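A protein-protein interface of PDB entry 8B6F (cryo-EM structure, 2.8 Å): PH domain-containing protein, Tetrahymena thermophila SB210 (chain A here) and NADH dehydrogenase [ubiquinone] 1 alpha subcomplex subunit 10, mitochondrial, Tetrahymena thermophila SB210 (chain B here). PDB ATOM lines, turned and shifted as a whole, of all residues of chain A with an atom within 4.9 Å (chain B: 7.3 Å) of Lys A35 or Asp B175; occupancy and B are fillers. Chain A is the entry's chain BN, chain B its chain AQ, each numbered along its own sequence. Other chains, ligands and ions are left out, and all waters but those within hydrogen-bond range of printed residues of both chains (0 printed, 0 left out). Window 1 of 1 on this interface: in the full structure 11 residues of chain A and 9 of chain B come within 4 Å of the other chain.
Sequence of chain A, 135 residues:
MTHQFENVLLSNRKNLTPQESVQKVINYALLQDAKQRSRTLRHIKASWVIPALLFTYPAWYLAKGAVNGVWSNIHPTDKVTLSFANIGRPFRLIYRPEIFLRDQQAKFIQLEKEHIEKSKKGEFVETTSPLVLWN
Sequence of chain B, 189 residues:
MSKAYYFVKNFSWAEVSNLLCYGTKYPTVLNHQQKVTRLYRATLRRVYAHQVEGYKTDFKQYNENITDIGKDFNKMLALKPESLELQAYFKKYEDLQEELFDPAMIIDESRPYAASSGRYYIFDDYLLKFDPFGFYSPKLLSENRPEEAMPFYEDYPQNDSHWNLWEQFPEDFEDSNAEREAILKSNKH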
ATOM      1  N   LEU A  31     -18.485  25.921 -24.283  1.00  0.00           N
ATOM      2  CA  LEU A  31     -19.805  25.305 -24.236  1.00  0.00           C
ATOM      3  C   LEU A  31     -20.721  26.044 -23.268  1.00  0.00           C
ATOM      4  O   LEU A  31     -21.883  26.324 -23.584  1.00  0.00           O
ATOM      5  CB  LEU A  31     -19.676  23.834 -23.842  1.00  0.00           C
ATOM      6  CG  LEU A  31     -20.977  23.033 -23.783  1.00  0.00           C
ATOM      7  CD1 LEU A  31     -21.719  23.078 -25.108  1.00  0.00           C
ATOM      8  CD2 LEU A  31     -20.686  21.597 -23.381  1.00  0.00           C
ATOM      9  N   GLN A  32     -20.213  26.369 -22.079  1.00  0.00           N
ATOM     10  CA  GLN A  32     -21.028  27.078 -21.099  1.00  0.00           C
ATOM     11  C   GLN A  32     -21.391  28.472 -21.592  1.00  0.00           C
ATOM     12  O   GLN A  32     -22.515  28.942 -21.377  1.00  0.00           O
ATOM     13  CB  GLN A  32     -20.298  27.150 -19.760  1.00  0.00           C
ATOM     14  CG  GLN A  32     -20.008  25.791 -19.149  1.00  0.00           C
ATOM     15  CD  GLN A  32     -21.266  24.990 -18.888  1.00  0.00           C
ATOM     16  OE1 GLN A  32     -22.313  25.545 -18.560  1.00  0.00           O
ATOM     17  NE2 GLN A  32     -21.173  23.676 -19.041  1.00  0.00           N
ATOM     18  N   ASP A  33     -20.454  29.147 -22.260  1.00  0.00           N
ATOM     19  CA  ASP A  33     -20.746  30.460 -22.822  1.00  0.00           C
ATOM     20  C   ASP A  33     -21.823  30.372 -23.893  1.00  0.00           C
ATOM     21  O   ASP A  33     -22.684  31.252 -23.991  1.00  0.00           O
ATOM     22  CB  ASP A  33     -19.474  31.080 -23.397  1.00  0.00           C
ATOM     23  CG  ASP A  33     -18.431  31.356 -22.337  1.00  0.00           C
ATOM     24  OD1 ASP A  33     -18.817  31.688 -21.196  1.00  0.00           O
ATOM     25  OD2 ASP A  33     -17.226  31.245 -22.642  1.00  0.00           O
ATOM     26  N   ALA A  34     -21.790  29.318 -24.709  1.00  0.00           N
ATOM     27  CA  ALA A  34     -22.840  29.134 -25.702  1.00  0.00           C
ATOM     28  C   ALA A  34     -24.199  28.944 -25.041  1.00  0.00           C
ATOM     29  O   ALA A  34     -25.202  29.507 -25.493  1.00  0.00           O
ATOM     30  CB  ALA A  34     -22.511  27.945 -26.599  1.00  0.00           C
ATOM     31  N   LYS A  35     -24.256  28.148 -23.971  1.00  0.00           N
ATOM     32  CA  LYS A  35     -25.519  27.967 -23.264  1.00  0.00           C
ATOM     33  C   LYS A  35     -26.022  29.292 -22.706  1.00  0.00           C
ATOM     34  O   LYS A  35     -27.208  29.617 -22.830  1.00  0.00           O
ATOM     35  CB  LYS A  35     -25.353  26.944 -22.142  1.00  0.00           C
ATOM     36  CG  LYS A  35     -25.030  25.541 -22.619  1.00  0.00           C
ATOM     37  CD  LYS A  35     -24.899  24.587 -21.443  1.00  0.00           C
ATOM     38  CE  LYS A  35     -24.559  23.181 -21.900  1.00  0.00           C
ATOM     39  NZ  LYS A  35     -24.351  22.267 -20.744  1.00  0.00           N
ATOM     40  N   GLN A  36     -25.133  30.071 -22.088  1.00  0.00           N
ATOM     41  CA  GLN A  36     -25.534  31.364 -21.543  1.00  0.00           C
ATOM     42  C   GLN A  36     -26.011  32.290 -22.650  1.00  0.00           C
ATOM     43  O   GLN A  36     -26.998  33.016 -22.486  1.00  0.00           O
ATOM     44  CB  GLN A  36     -24.370  31.998 -20.783  1.00  0.00           C
ATOM     45  CG  GLN A  36     -24.690  33.360 -20.185  1.00  0.00           C
ATOM     46  CD  GLN A  36     -23.480  34.009 -19.554  1.00  0.00           C
ATOM     47  OE1 GLN A  36     -22.371  33.487 -19.633  1.00  0.00           O
ATOM     48  NE2 GLN A  36     -23.687  35.156 -18.922  1.00  0.00           N
ATOM     49  N   ARG A  37     -25.320  32.272 -23.787  1.00  0.00           N
ATOM     50  CA  ARG A  37     -25.737  33.071 -24.931  1.00  0.00           C
ATOM     51  C   ARG A  37     -27.143  32.695 -25.373  1.00  0.00           C
ATOM     52  O   ARG A  37     -27.971  33.568 -25.653  1.00  0.00           O
ATOM     53  CB  ARG A  37     -24.745  32.868 -26.072  1.00  0.00           C
ATOM     54  CG  ARG A  37     -24.460  34.091 -26.906  1.00  0.00           C
ATOM     55  CD  ARG A  37     -23.458  33.727 -27.976  1.00  0.00           C
ATOM     56  NE  ARG A  37     -22.190  33.297 -27.399  1.00  0.00           N
ATOM     57  CZ  ARG A  37     -21.314  32.510 -28.007  1.00  0.00           C
ATOM     58  NH1 ARG A  37     -21.543  32.025 -29.216  1.00  0.00           N
ATOM     59  NH2 ARG A  37     -20.183  32.195 -27.384  1.00  0.00           N
ATOM     60  N   SER A  38     -27.427  31.395 -25.449  1.00  0.00           N
ATOM     61  CA  SER A  38     -28.763  30.953 -25.828  1.00  0.00           C
ATOM     62  C   SER A  38     -29.814  31.449 -24.843  1.00  0.00           C
ATOM     63  O   SER A  38     -30.878  31.926 -25.249  1.00  0.00           O
ATOM     64  CB  SER A  38     -28.792  29.427 -25.918  1.00  0.00           C
ATOM     65  OG  SER A  38     -30.089  28.957 -26.236  1.00  0.00           O
ATOM     66  N   ARG A  39     -29.536  31.342 -23.541  1.00  0.00           N
ATOM     67  CA  ARG A  39     -30.513  31.766 -22.541  1.00  0.00           C
ATOM     68  C   ARG A  39     -30.798  33.260 -22.645  1.00  0.00           C
ATOM     69  O   ARG A  39     -31.958  33.683 -22.651  1.00  0.00           O
ATOM     70  CB  ARG A  39     -30.018  31.414 -21.139  1.00  0.00           C
ATOM     71  CG  ARG A  39     -30.009  29.924 -20.836  1.00  0.00           C
ATOM     72  CD  ARG A  39     -29.740  29.666 -19.362  1.00  0.00           C
ATOM     73  NE  ARG A  39     -28.438  30.173 -18.944  1.00  0.00           N
ATOM     74  CZ  ARG A  39     -27.305  29.488 -19.009  1.00  0.00           C
ATOM     75  NH1 ARG A  39     -27.267  28.252 -19.477  1.00  0.00           N
ATOM     76  NH2 ARG A  39     -26.179  30.058 -18.592  1.00  0.00           N
ATOM     77  N   ARG A  42     -32.830  34.068 -25.676  1.00  0.00           N
ATOM     78  CA  ARG A  42     -34.229  33.707 -25.485  1.00  0.00           C
ATOM     79  C   ARG A  42     -34.957  34.752 -24.650  1.00  0.00           C
ATOM     80  O   ARG A  42     -36.106  35.100 -24.945  1.00  0.00           O
ATOM     81  CB  ARG A  42     -34.326  32.334 -24.827  1.00  0.00           C
ATOM     82  CG  ARG A  42     -35.729  31.761 -24.807  1.00  0.00           C
ATOM     83  CD  ARG A  42     -35.788  30.497 -23.976  1.00  0.00           C
ATOM     84  NE  ARG A  42     -34.611  29.661 -24.175  1.00  0.00           N
ATOM     85  CZ  ARG A  42     -34.426  28.856 -25.212  1.00  0.00           C
ATOM     86  NH1 ARG A  42     -35.330  28.746 -26.172  1.00  0.00           N
ATOM     87  NH2 ARG A  42     -33.306  28.144 -25.289  1.00  0.00           N
ATOM     88  N   PHE B 169     -28.927  28.477 -33.194  1.00  0.00           N
ATOM     89  CA  PHE B 169     -28.547  27.337 -32.375  1.00  0.00           C
ATOM     90  C   PHE B 169     -29.223  26.080 -32.897  1.00  0.00           C
ATOM     91  O   PHE B 169     -30.278  26.156 -33.534  1.00  0.00           O
ATOM     92  CB  PHE B 169     -28.937  27.555 -30.905  1.00  0.00           C
ATOM     93  CG  PHE B 169     -28.292  28.757 -30.281  1.00  0.00           C
ATOM     94  CD1 PHE B 169     -27.055  28.655 -29.668  1.00  0.00           C
ATOM     95  CD2 PHE B 169     -28.920  29.989 -30.307  1.00  0.00           C
ATOM     96  CE1 PHE B 169     -26.456  29.758 -29.094  1.00  0.00           C
ATOM     97  CE2 PHE B 169     -28.326  31.097 -29.734  1.00  0.00           C
ATOM     98  CZ  PHE B 169     -27.093  30.981 -29.126  1.00  0.00           C
ATOM     99  N   ASP B 172     -33.594  22.035 -30.415  1.00  0.00           N
ATOM    100  CA  ASP B 172     -33.576  21.335 -29.132  1.00  0.00           C
ATOM    101  C   ASP B 172     -32.195  21.418 -28.485  1.00  0.00           C
ATOM    102  O   ASP B 172     -31.694  20.446 -27.918  1.00  0.00           O
ATOM    103  CB  ASP B 172     -34.016  19.878 -29.294  1.00  0.00           C
ATOM    104  CG  ASP B 172     -35.421  19.752 -29.851  1.00  0.00           C
ATOM    105  OD1 ASP B 172     -36.054  20.797 -30.111  1.00  0.00           O
ATOM    106  OD2 ASP B 172     -35.894  18.611 -30.027  1.00  0.00           O
ATOM    107  N   PHE B 173     -31.576  22.592 -28.575  1.00  0.00           N
ATOM    108  CA  PHE B 173     -30.272  22.805 -27.963  1.00  0.00           C
ATOM    109  C   PHE B 173     -30.416  22.912 -26.450  1.00  0.00           C
ATOM    110  O   PHE B 173     -31.260  23.659 -25.947  1.00  0.00           O
ATOM    111  CB  PHE B 173     -29.629  24.072 -28.529  1.00  0.00           C
ATOM    112  CG  PHE B 173     -28.283  24.386 -27.948  1.00  0.00           C
ATOM    113  CD1 PHE B 173     -27.175  23.627 -28.284  1.00  0.00           C
ATOM    114  CD2 PHE B 173     -28.119  25.455 -27.086  1.00  0.00           C
ATOM    115  CE1 PHE B 173     -25.934  23.918 -27.757  1.00  0.00           C
ATOM    116  CE2 PHE B 173     -26.880  25.752 -26.557  1.00  0.00           C
ATOM    117  CZ  PHE B 173     -25.786  24.984 -26.894  1.00  0.00           C
ATOM    118  N   GLU B 174     -29.589  22.163 -25.725  1.00  0.00           N
ATOM    119  CA  GLU B 174     -29.618  22.183 -24.269  1.00  0.00           C
ATOM    120  C   GLU B 174     -28.849  23.397 -23.768  1.00  0.00           C
ATOM    121  O   GLU B 174     -27.661  23.553 -24.068  1.00  0.00           O
ATOM    122  CB  GLU B 174     -29.016  20.895 -23.710  1.00  0.00           C
ATOM    123  CG  GLU B 174     -28.983  20.831 -22.190  1.00  0.00           C
ATOM    124  CD  GLU B 174     -28.297  19.579 -21.677  1.00  0.00           C
ATOM    125  OE1 GLU B 174     -27.932  18.719 -22.505  1.00  0.00           O
ATOM    126  OE2 GLU B 174     -28.118  19.459 -20.447  1.00  0.00           O
ATOM    127  N   ASP B 175     -29.524  24.258 -23.000  1.00  0.00           N
ATOM    128  CA  ASP B 175     -28.899  25.485 -22.523  1.00  0.00           C
ATOM    129  C   ASP B 175     -29.226  25.774 -21.060  1.00  0.00           C
ATOM    130  O   ASP B 175     -29.085  26.921 -20.622  1.00  0.00           O
ATOM    131  CB  ASP B 175     -29.320  26.675 -23.389  1.00  0.00           C
ATOM    132  CG  ASP B 175     -30.821  26.879 -23.407  1.00  0.00           C
ATOM    133  OD1 ASP B 175     -31.559  25.906 -23.147  1.00  0.00           O
ATOM    134  OD2 ASP B 175     -31.266  28.011 -23.687  1.00  0.00           O
ATOM    135  N   SER B 176     -29.655  24.774 -20.298  1.00  0.00           N
ATOM    136  CA  SER B 176     -29.947  24.990 -18.888  1.00  0.00           C
ATOM    137  C   SER B 176     -28.671  25.350 -18.136  1.00  0.00           C
ATOM    138  O   SER B 176     -27.580  24.862 -18.444  1.00  0.00           O
ATOM    139  CB  SER B 176     -30.585  23.744 -18.276  1.00  0.00           C
ATOM    140  OG  SER B 176     -29.727  22.622 -18.393  1.00  0.00           O
ATOM    141  N   ASN B 177     -28.819  26.213 -17.133  1.00  0.00           N
ATOM    142  CA  ASN B 177     -27.686  26.694 -16.343  1.00  0.00           C
ATOM    143  C   ASN B 177     -27.263  25.587 -15.382  1.00  0.00           C
ATOM    144  O   ASN B 177     -27.591  25.580 -14.193  1.00  0.00           O
ATOM    145  CB  ASN B 177     -28.059  27.971 -15.603  1.00  0.00           C
ATOM    146  CG  ASN B 177     -26.851  28.731 -15.109  1.00  0.00           C
ATOM    147  OD1 ASN B 177     -25.777  28.164 -14.922  1.00  0.00           O
ATOM    148  ND2 ASN B 177     -27.024  30.027 -14.886  1.00  0.00           N
ATOM    149  N   ALA B 178     -26.516  24.624 -15.925  1.00  0.00           N
ATOM    150  CA  ALA B 178     -26.122  23.457 -15.143  1.00  0.00           C
ATOM    151  C   ALA B 178     -25.211  23.845 -13.984  1.00  0.00           C
ATOM    152  O   ALA B 178     -25.320  23.286 -12.887  1.00  0.00           O
ATOM    153  CB  ALA B 178     -25.435  22.433 -16.043  1.00  0.00           C
ATOM    154  N   GLU B 179     -24.301  24.793 -14.208  1.00  0.00           N
ATOM    155  CA  GLU B 179     -23.401  25.219 -13.140  1.00  0.00           C
ATOM    156  C   GLU B 179     -24.181  25.790 -11.963  1.00  0.00           C
ATOM    157  O   GLU B 179     -23.961  25.403 -10.811  1.00  0.00           O
ATOM    158  CB  GLU B 179     -22.408  26.251 -13.667  1.00  0.00           C
ATOM    159  CG  GLU B 179     -21.490  25.732 -14.758  1.00  0.00           C
ATOM    160  CD  GLU B 179     -20.615  26.824 -15.337  1.00  0.00           C
ATOM    161  OE1 GLU B 179     -21.012  28.005 -15.266  1.00  0.00           O
ATOM    162  OE2 GLU B 179     -19.527  26.505 -15.856  1.00  0.00           O
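OD2 of Asp B175 sits at hydrogen-bond distance from OG of Ser A38 (3.0 Å).
O of Asp B175 is in hydrogen-bond range of NH1 of Arg A39, at 2.5 Å.
The backbone NH (N) of Asn B177 lies close to the guanidinium group (NH1) of Arg A39 (3.5 Å).
The side-chain carboxylate of Asp B175 lies within salt-bridge range of the guanidinium group of Arg A42 (2.6 Å).
OG of Ser A38 sits at hydrogen-bond distance from NH2 of Arg A42.
Gln A32 touches Glu B179.
Ala A34 touches Phe B169 (O to CE1, 3.8 Å).
Lys A35 touches Glu B174 (CG to O, 3.6 Å).
Lys A35 touches Asp B175 (O to CB, 3.7 Å).
Ser A38 touches Phe B169.
Ser B176 touches Arg A39.
Leu A31 touches none of the printed residues of chain B.
Lys A35 touches just these residues of chain B: Glu B174 (3.6 Å) and Asp B175 (3.7 Å).
Asp B172 touches none of the printed residues of chain A.
Of the printed residues of chain A, Ser B176 touches Arg A39.
Of the printed residues of chain A, Glu B179 touches Gln A32 (3.4 Å).
The nearest printed residue of chain A that does not touch Asp B175 is Gln A36 (5.3 Å).
The nearest printed residue of chain B that does not touch Arg A39 is Ala B178 (5.1 Å).
Of the 9 printed residues of chain B, 6 touch a printed residue of chain A.
Of the 10 printed residues of chain A, 6 touch a printed residue of chain B.
Along chain A the printed residues that touch a printed residue of chain B span positions 32 to 42.
Among the printed residues, 10 pairs touch across the chains.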
